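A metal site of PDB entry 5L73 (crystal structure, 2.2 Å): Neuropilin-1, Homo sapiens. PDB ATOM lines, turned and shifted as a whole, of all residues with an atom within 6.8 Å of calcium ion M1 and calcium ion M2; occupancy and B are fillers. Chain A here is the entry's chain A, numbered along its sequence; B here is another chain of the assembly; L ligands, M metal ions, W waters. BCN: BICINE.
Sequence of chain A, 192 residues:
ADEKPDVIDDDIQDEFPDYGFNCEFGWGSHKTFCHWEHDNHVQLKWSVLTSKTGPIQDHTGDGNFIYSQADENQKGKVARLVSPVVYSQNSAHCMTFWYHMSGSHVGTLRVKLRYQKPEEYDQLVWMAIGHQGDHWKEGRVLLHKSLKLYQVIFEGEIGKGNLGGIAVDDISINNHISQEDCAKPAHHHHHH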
ATOM      1  N   CYS A  23      15.041   0.400  -3.870  1.00  0.00           N
ATOM      2  CA  CYS A  23      15.009   0.177  -2.434  1.00  0.00           C
ATOM      3  C   CYS A  23      16.360   0.285  -1.743  1.00  0.00           C
ATOM      4  O   CYS A  23      17.300  -0.417  -2.096  1.00  0.00           O
ATOM      5  CB  CYS A  23      14.386  -1.178  -2.100  1.00  0.00           C
ATOM      6  SG  CYS A  23      13.772  -1.312  -0.392  1.00  0.00           S
ATOM      7  N   GLU A  24      16.427   1.181  -0.759  1.00  0.00           N
ATOM      8  CA  GLU A  24      17.562   1.367   0.114  1.00  0.00           C
ATOM      9  C   GLU A  24      17.366   0.648   1.477  1.00  0.00           C
ATOM     10  O   GLU A  24      18.270   0.656   2.306  1.00  0.00           O
ATOM     11  CB  GLU A  24      17.777   2.889   0.361  1.00  0.00           C
ATOM     12  CG  GLU A  24      18.782   3.514  -0.588  1.00  0.00           C
ATOM     13  CD  GLU A  24      20.238   3.138  -0.236  1.00  0.00           C
ATOM     14  OE1 GLU A  24      21.174   3.762  -0.763  1.00  0.00           O
ATOM     15  OE2 GLU A  24      20.470   2.229   0.576  1.00  0.00           O
ATOM     16  N   PHE A  25      16.164   0.089   1.679  1.00  0.00           N
ATOM     17  CA  PHE A  25      15.746  -0.649   2.884  1.00  0.00           C
ATOM     18  C   PHE A  25      15.514   0.215   4.112  1.00  0.00           C
ATOM     19  O   PHE A  25      15.519  -0.281   5.235  1.00  0.00           O
ATOM     20  CB  PHE A  25      16.635  -1.877   3.135  1.00  0.00           C
ATOM     21  CG  PHE A  25      16.690  -2.783   1.948  1.00  0.00           C
ATOM     22  CD1 PHE A  25      15.601  -3.592   1.615  1.00  0.00           C
ATOM     23  CD2 PHE A  25      17.775  -2.755   1.081  1.00  0.00           C
ATOM     24  CE1 PHE A  25      15.640  -4.418   0.500  1.00  0.00           C
ATOM     25  CE2 PHE A  25      17.818  -3.563  -0.047  1.00  0.00           C
ATOM     26  CZ  PHE A  25      16.742  -4.389  -0.345  1.00  0.00           C
ATOM     27  N   GLY A  26      15.251   1.507   3.863  1.00  0.00           N
ATOM     28  CA  GLY A  26      14.906   2.476   4.852  1.00  0.00           C
ATOM     29  C   GLY A  26      16.053   3.160   5.531  1.00  0.00           C
ATOM     30  O   GLY A  26      17.172   3.200   5.014  1.00  0.00           O
ATOM     31  N   SER A  51      22.576  -0.154  10.338  1.00  0.00           N
ATOM     32  CA  SER A  51      24.041  -0.066  10.410  1.00  0.00           C
ATOM     33  C   SER A  51      24.381   0.454  11.782  1.00  0.00           C
ATOM     34  O   SER A  51      23.985   1.572  12.130  1.00  0.00           O
ATOM     35  CB  SER A  51      24.602   0.884   9.353  1.00  0.00           C
ATOM     36  OG  SER A  51      24.394   0.402   8.020  1.00  0.00           O
ATOM     37  N   GLN A  57      28.231  -2.382   6.847  1.00  0.00           N
ATOM     38  CA  GLN A  57      27.328  -1.279   7.043  1.00  0.00           C
ATOM     39  C   GLN A  57      27.087  -0.496   5.759  1.00  0.00           C
ATOM     40  O   GLN A  57      27.907  -0.526   4.814  1.00  0.00           O
ATOM     41  CB  GLN A  57      27.883  -0.316   8.119  1.00  0.00           C
ATOM     42  CG  GLN A  57      28.103  -0.898   9.501  1.00  0.00           C
ATOM     43  CD  GLN A  57      28.547   0.167  10.497  1.00  0.00           C
ATOM     44  OE1 GLN A  57      27.901   1.236  10.620  1.00  0.00           O
ATOM     45  NE2 GLN A  57      29.660  -0.070  11.173  1.00  0.00           N
ATOM     46  N   ASP A  58      25.952   0.183   5.735  1.00  0.00           N
ATOM     47  CA  ASP A  58      25.661   1.192   4.757  1.00  0.00           C
ATOM     48  C   ASP A  58      26.278   2.485   5.311  1.00  0.00           C
ATOM     49  O   ASP A  58      25.564   3.386   5.737  1.00  0.00           O
ATOM     50  CB  ASP A  58      24.145   1.304   4.563  1.00  0.00           C
ATOM     51  CG  ASP A  58      23.754   2.267   3.459  1.00  0.00           C
ATOM     52  OD1 ASP A  58      24.666   2.844   2.791  1.00  0.00           O
ATOM     53  OD2 ASP A  58      22.535   2.426   3.219  1.00  0.00           O
ATOM     54  N   HIS A  59      27.617   2.555   5.294  1.00  0.00           N
ATOM     55  CA  HIS A  59      28.390   3.562   6.062  1.00  0.00           C
ATOM     56  C   HIS A  59      28.103   4.951   5.540  1.00  0.00           C
ATOM     57  O   HIS A  59      28.005   5.896   6.291  1.00  0.00           O
ATOM     58  CB  HIS A  59      29.915   3.377   5.929  1.00  0.00           C
ATOM     59  CG  HIS A  59      30.447   2.147   6.594  1.00  0.00           C
ATOM     60  ND1 HIS A  59      30.858   2.116   7.909  1.00  0.00           N
ATOM     61  CD2 HIS A  59      30.679   0.909   6.093  1.00  0.00           C
ATOM     62  CE1 HIS A  59      31.308   0.906   8.205  1.00  0.00           C
ATOM     63  NE2 HIS A  59      31.210   0.158   7.122  1.00  0.00           N
ATOM     64  N   THR A  60      27.969   5.047   4.230  1.00  0.00           N
ATOM     65  CA  THR A  60      27.961   6.293   3.541  1.00  0.00           C
ATOM     66  C   THR A  60      26.602   7.003   3.718  1.00  0.00           C
ATOM     67  O   THR A  60      26.564   8.227   3.763  1.00  0.00           O
ATOM     68  CB  THR A  60      28.391   6.056   2.075  1.00  0.00           C
ATOM     69  OG1 THR A  60      29.681   5.387   2.077  1.00  0.00           O
ATOM     70  CG2 THR A  60      28.502   7.350   1.336  1.00  0.00           C
ATOM     71  N   GLY A  61      25.515   6.255   3.838  1.00  0.00           N
ATOM     72  CA  GLY A  61      24.213   6.835   4.210  1.00  0.00           C
ATOM     73  C   GLY A  61      23.799   6.732   5.679  1.00  0.00           C
ATOM     74  O   GLY A  61      22.761   7.300   6.042  1.00  0.00           O
ATOM     75  N   ASP A  62      24.584   6.044   6.507  1.00  0.00           N
ATOM     76  CA  ASP A  62      24.164   5.583   7.872  1.00  0.00           C
ATOM     77  C   ASP A  62      22.863   4.782   7.821  1.00  0.00           C
ATOM     78  O   ASP A  62      21.997   4.930   8.697  1.00  0.00           O
ATOM     79  CB  ASP A  62      23.939   6.744   8.838  1.00  0.00           C
ATOM     80  CG  ASP A  62      24.990   7.773   8.750  1.00  0.00           C
ATOM     81  OD1 ASP A  62      26.178   7.387   8.873  1.00  0.00           O
ATOM     82  OD2 ASP A  62      24.625   8.983   8.549  1.00  0.00           O
ATOM     83  N   GLY A  63      22.732   3.939   6.812  1.00  0.00           N
ATOM     84  CA  GLY A  63      21.434   3.434   6.413  1.00  0.00           C
ATOM     85  C   GLY A  63      21.211   1.995   6.798  1.00  0.00           C
ATOM     86  O   GLY A  63      21.912   1.441   7.649  1.00  0.00           O
ATOM     87  N   ASN A  64      20.203   1.406   6.185  1.00  0.00           N
ATOM     88  CA  ASN A  64      19.862   0.029   6.425  1.00  0.00           C
ATOM     89  C   ASN A  64      20.305  -0.793   5.236  1.00  0.00           C
ATOM     90  O   ASN A  64      20.681  -0.249   4.199  1.00  0.00           O
ATOM     91  CB  ASN A  64      18.368  -0.121   6.674  1.00  0.00           C
ATOM     92  CG  ASN A  64      17.889   0.583   7.959  1.00  0.00           C
ATOM     93  OD1 ASN A  64      18.685   0.903   8.868  1.00  0.00           O
ATOM     94  ND2 ASN A  64      16.581   0.822   8.028  1.00  0.00           N
ATOM     95  N   PHE A  65      20.325  -2.112   5.425  1.00  0.00           N
ATOM     96  CA  PHE A  65      20.568  -3.075   4.373  1.00  0.00           C
ATOM     97  C   PHE A  65      19.893  -4.405   4.709  1.00  0.00           C
ATOM     98  O   PHE A  65      19.353  -4.554   5.822  1.00  0.00           O
ATOM     99  CB  PHE A  65      22.088  -3.248   4.162  1.00  0.00           C
ATOM    100  CG  PHE A  65      22.822  -3.732   5.380  1.00  0.00           C
ATOM    101  CD1 PHE A  65      23.264  -2.823   6.340  1.00  0.00           C
ATOM    102  CD2 PHE A  65      23.084  -5.081   5.551  1.00  0.00           C
ATOM    103  CE1 PHE A  65      23.900  -3.273   7.489  1.00  0.00           C
ATOM    104  CE2 PHE A  65      23.747  -5.535   6.680  1.00  0.00           C
ATOM    105  CZ  PHE A  65      24.169  -4.639   7.647  1.00  0.00           C
ATOM    106  N   ILE A  66      19.946  -5.357   3.787  1.00  0.00           N
ATOM    107  CA  ILE A  66      19.418  -6.712   4.029  1.00  0.00           C
ATOM    108  C   ILE A  66      20.522  -7.735   4.174  1.00  0.00           C
ATOM    109  O   ILE A  66      21.598  -7.564   3.621  1.00  0.00           O
ATOM    110  CB  ILE A  66      18.338  -7.153   3.025  1.00  0.00           C
ATOM    111  CG1 ILE A  66      18.873  -7.245   1.606  1.00  0.00           C
ATOM    112  CG2 ILE A  66      17.176  -6.181   3.053  1.00  0.00           C
ATOM    113  CD1 ILE A  66      17.905  -7.911   0.633  1.00  0.00           C
ATOM    114  N   TRP A  98      24.229  -3.470  -4.551  1.00  0.00           N
ATOM    115  CA  TRP A  98      25.451  -3.683  -3.854  1.00  0.00           C
ATOM    116  C   TRP A  98      25.350  -4.937  -3.025  1.00  0.00           C
ATOM    117  O   TRP A  98      24.296  -5.262  -2.536  1.00  0.00           O
ATOM    118  CB  TRP A  98      25.780  -2.486  -2.953  1.00  0.00           C
ATOM    119  CG  TRP A  98      26.111  -1.275  -3.744  1.00  0.00           C
ATOM    120  CD1 TRP A  98      25.214  -0.404  -4.322  1.00  0.00           C
ATOM    121  CD2 TRP A  98      27.414  -0.772  -4.067  1.00  0.00           C
ATOM    122  NE1 TRP A  98      25.883   0.585  -4.999  1.00  0.00           N
ATOM    123  CE2 TRP A  98      27.221   0.393  -4.841  1.00  0.00           C
ATOM    124  CE3 TRP A  98      28.706  -1.199  -3.782  1.00  0.00           C
ATOM    125  CZ2 TRP A  98      28.303   1.154  -5.336  1.00  0.00           C
ATOM    126  CZ3 TRP A  98      29.765  -0.458  -4.249  1.00  0.00           C
ATOM    127  CH2 TRP A  98      29.565   0.701  -5.026  1.00  0.00           C
ATOM    128  N   TRP A 136      32.104  -4.058   0.088  1.00  0.00           N
ATOM    129  CA  TRP A 136      30.956  -3.925  -0.781  1.00  0.00           C
ATOM    130  C   TRP A 136      31.372  -3.869  -2.259  1.00  0.00           C
ATOM    131  O   TRP A 136      32.309  -3.130  -2.630  1.00  0.00           O
ATOM    132  CB  TRP A 136      30.206  -2.627  -0.425  1.00  0.00           C
ATOM    133  CG  TRP A 136      29.439  -2.654   0.867  1.00  0.00           C
ATOM    134  CD1 TRP A 136      29.833  -2.142   2.062  1.00  0.00           C
ATOM    135  CD2 TRP A 136      28.155  -3.235   1.080  1.00  0.00           C
ATOM    136  NE1 TRP A 136      28.859  -2.354   3.014  1.00  0.00           N
ATOM    137  CE2 TRP A 136      27.818  -3.032   2.430  1.00  0.00           C
ATOM    138  CE3 TRP A 136      27.251  -3.903   0.255  1.00  0.00           C
ATOM    139  CZ2 TRP A 136      26.612  -3.448   2.970  1.00  0.00           C
ATOM    140  CZ3 TRP A 136      26.046  -4.337   0.795  1.00  0.00           C
ATOM    141  CH2 TRP A 136      25.736  -4.085   2.149  1.00  0.00           C
ATOM    142  N   VAL A 168      23.043  -7.321   1.152  1.00  0.00           N
ATOM    143  CA  VAL A 168      22.672  -6.610  -0.073  1.00  0.00           C
ATOM    144  C   VAL A 168      22.093  -5.249   0.307  1.00  0.00           C
ATOM    145  O   VAL A 168      21.517  -5.083   1.415  1.00  0.00           O
ATOM    146  CB  VAL A 168      21.624  -7.415  -0.869  1.00  0.00           C
ATOM    147  CG1 VAL A 168      21.117  -6.627  -2.063  1.00  0.00           C
ATOM    148  CG2 VAL A 168      22.178  -8.777  -1.321  1.00  0.00           C
ATOM    149  N   ASP A 169      22.260  -4.274  -0.595  1.00  0.00           N
ATOM    150  CA  ASP A 169      21.685  -2.953  -0.404  1.00  0.00           C
ATOM    151  C   ASP A 169      21.474  -2.226  -1.710  1.00  0.00           C
ATOM    152  O   ASP A 169      22.028  -2.573  -2.755  1.00  0.00           O
ATOM    153  CB  ASP A 169      22.627  -2.097   0.473  1.00  0.00           C
ATOM    154  CG  ASP A 169      21.920  -0.925   1.177  1.00  0.00           C
ATOM    155  OD1 ASP A 169      20.682  -0.866   1.155  1.00  0.00           O
ATOM    156  OD2 ASP A 169      22.613  -0.044   1.772  1.00  0.00           O
ATOM    157  N   ASP A 170      20.638  -1.192  -1.625  1.00  0.00           N
ATOM    158  CA  ASP A 170      20.608  -0.154  -2.619  1.00  0.00           C
ATOM    159  C   ASP A 170      20.353  -0.708  -4.019  1.00  0.00           C
ATOM    160  O   ASP A 170      21.156  -0.525  -4.934  1.00  0.00           O
ATOM    161  CB  ASP A 170      21.921   0.636  -2.541  1.00  0.00           C
ATOM    162  CG  ASP A 170      21.885   1.916  -3.362  1.00  0.00           C
ATOM    163  OD1 ASP A 170      20.797   2.299  -3.841  1.00  0.00           O
ATOM    164  OD2 ASP A 170      22.956   2.530  -3.500  1.00  0.00           O
ATOM    165  N   GLU B 138      25.590  11.917  -3.621  1.00  0.00           N
ATOM    166  CA  GLU B 138      26.766  11.227  -3.116  1.00  0.00           C
ATOM    167  C   GLU B 138      27.812  11.346  -4.209  1.00  0.00           C
ATOM    168  O   GLU B 138      27.530  11.026  -5.339  1.00  0.00           O
ATOM    169  CB  GLU B 138      26.428   9.746  -2.801  1.00  0.00           C
ATOM    170  CG  GLU B 138      27.561   8.799  -2.360  1.00  0.00           C
ATOM    171  CD  GLU B 138      27.087   7.372  -1.968  1.00  0.00           C
ATOM    172  OE1 GLU B 138      27.929   6.414  -2.025  1.00  0.00           O
ATOM    173  OE2 GLU B 138      25.894   7.166  -1.592  1.00  0.00           O
ATOM    174  N   ARG B 140      31.948  10.194  -5.099  1.00  0.00           N
ATOM    175  CA  ARG B 140      33.047   9.360  -4.644  1.00  0.00           C
ATOM    176  C   ARG B 140      34.244   9.453  -5.548  1.00  0.00           C
ATOM    177  O   ARG B 140      34.105   9.519  -6.753  1.00  0.00           O
ATOM    178  CB  ARG B 140      32.682   7.884  -4.569  1.00  0.00           C
ATOM    179  CG  ARG B 140      31.599   7.474  -3.614  1.00  0.00           C
ATOM    180  CD  ARG B 140      31.528   5.948  -3.605  1.00  0.00           C
ATOM    181  NE  ARG B 140      30.145   5.593  -3.783  1.00  0.00           N
ATOM    182  CZ  ARG B 140      29.584   4.948  -4.805  1.00  0.00           C
ATOM    183  NH1 ARG B 140      30.268   4.436  -5.819  1.00  0.00           N
ATOM    184  NH2 ARG B 140      28.285   4.783  -4.752  1.00  0.00           N
ATOM    185  N   ILE B 177      34.506  -0.097   0.525  1.00  0.00           N
ATOM    186  CA  ILE B 177      33.966  -0.068  -0.842  1.00  0.00           C
ATOM    187  C   ILE B 177      35.081  -0.548  -1.727  1.00  0.00           C
ATOM    188  O   ILE B 177      36.189  -0.066  -1.619  1.00  0.00           O
ATOM    189  CB  ILE B 177      33.550   1.353  -1.256  1.00  0.00           C
ATOM    190  CG1 ILE B 177      32.430   1.844  -0.349  1.00  0.00           C
ATOM    191  CG2 ILE B 177      33.081   1.399  -2.723  1.00  0.00           C
ATOM    192  CD1 ILE B 177      32.038   3.277  -0.585  1.00  0.00           C
HETATM  193  N1  BCN L   1      27.656   1.245  -0.074  1.00  0.00           N
HETATM  194  C1  BCN L   1      28.568   1.055   1.072  1.00  0.00           C
HETATM  195  C2  BCN L   1      28.598   2.327   1.870  1.00  0.00           C
HETATM  196  O21 BCN L   1      29.696   2.615   2.426  1.00  0.00           O
HETATM  197  O22 BCN L   1      27.557   3.017   1.960  1.00  0.00           O
HETATM  198  C3  BCN L   1      28.399   1.836  -1.221  1.00  0.00           C
HETATM  199  C4  BCN L   1      28.094   3.298  -1.391  1.00  0.00           C
HETATM  200  O4  BCN L   1      26.657   3.448  -1.460  1.00  0.00           O
HETATM  201  C5  BCN L   1      26.999  -0.029  -0.445  1.00  0.00           C
HETATM  202  C6  BCN L   1      25.967  -0.476   0.598  1.00  0.00           C
HETATM  203  O6  BCN L   1      25.049   0.604   0.781  1.00  0.00           O
HETATM  204 CA    CA M   1      20.664   1.175   2.521  1.00  0.00          CA
HETATM  205 CA    CA M   2      25.699   2.908   0.670  1.00  0.00          CA
HETATM  206  O   HOH W   1      19.570   2.834   3.694  1.00  0.00           O
HETATM  207  O   HOH W   2      23.731   2.751  -0.461  1.00  0.00           O
HETATM  208  O   HOH W   3      25.459   5.189   0.734  1.00  0.00           O
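Water W1 lies within hydrogen-bond range of the backbone carbonyl oxygen (O) of Gly 26 and the backbone NH (N) of Asn 64.
Water W3 bridges the side-chain carboxylate of Glu 138 of chain B (3.1 Å) and the backbone NH of Gly 61 (3.3 Å).
Water W2 bridges the side-chain carboxylate of Glu 24 (2.8 Å) and the side-chain carboxylate of Asp 170 (3.1 Å).
The backbone NH (N) of Thr 60 lies within hydrogen-bond range of an oxygen (O21) of the ligand (3.5 Å).
An oxygen (O21) of the ligand lies within hydrogen-bond range of the side-chain hydroxyl of Thr 60 (2.8 Å).
An oxygen (O4) of the ligand lies close to the side-chain carboxylate of Glu 138 of chain B (3.3 Å).
An oxygen (O22) of the ligand sits close to the backbone NH (N) of His 59, at 3.4 Å.
O22 of the ligand binds calcium ion M2 (2.3 Å).
Water W2 binds calcium ion M2.
Calcium ion M2 is bound by water W3.
The side-chain carboxylate (OD1) of Asp 58 binds calcium ion M2.
O4 of the ligand binds calcium ion M2 (2.4 Å).
O6 of the ligand binds calcium ion M2 (2.4 Å).
N1 of the ligand binds calcium ion M2, 2.7 Å away.
ND2 of Asn 64 is in hydrogen-bond range of O of Phe 25, at 3.2 Å.
The backbone NH of Gly 63 is in hydrogen-bond range of the backbone carbonyl oxygen of Asp 58 (3.1 Å).
The side-chain hydroxyl (OG) of Ser 51 lies within hydrogen-bond range of the backbone NH (N) of Asp 58 (2.8 Å).
The backbone carbonyl oxygen of Asp 169 is in hydrogen-bond range of the backbone NH of Trp 98.
Calcium ion M1 is bound by O of Asn 64 (2.2 Å), OE2 of Glu 24 (2.2 Å), water W1 (2.3 Å), OD2 of Asp 58 (2.4 Å), OD2 of Asp 169 (2.4 Å), OD1 of Asp 169 (2.5 Å) and O of Glu 24 (2.5 Å).
Calcium ion M1 has seven donor atoms within binding distance.
One residue has an atom within 4 Å of calcium ion M2: Asp 58.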
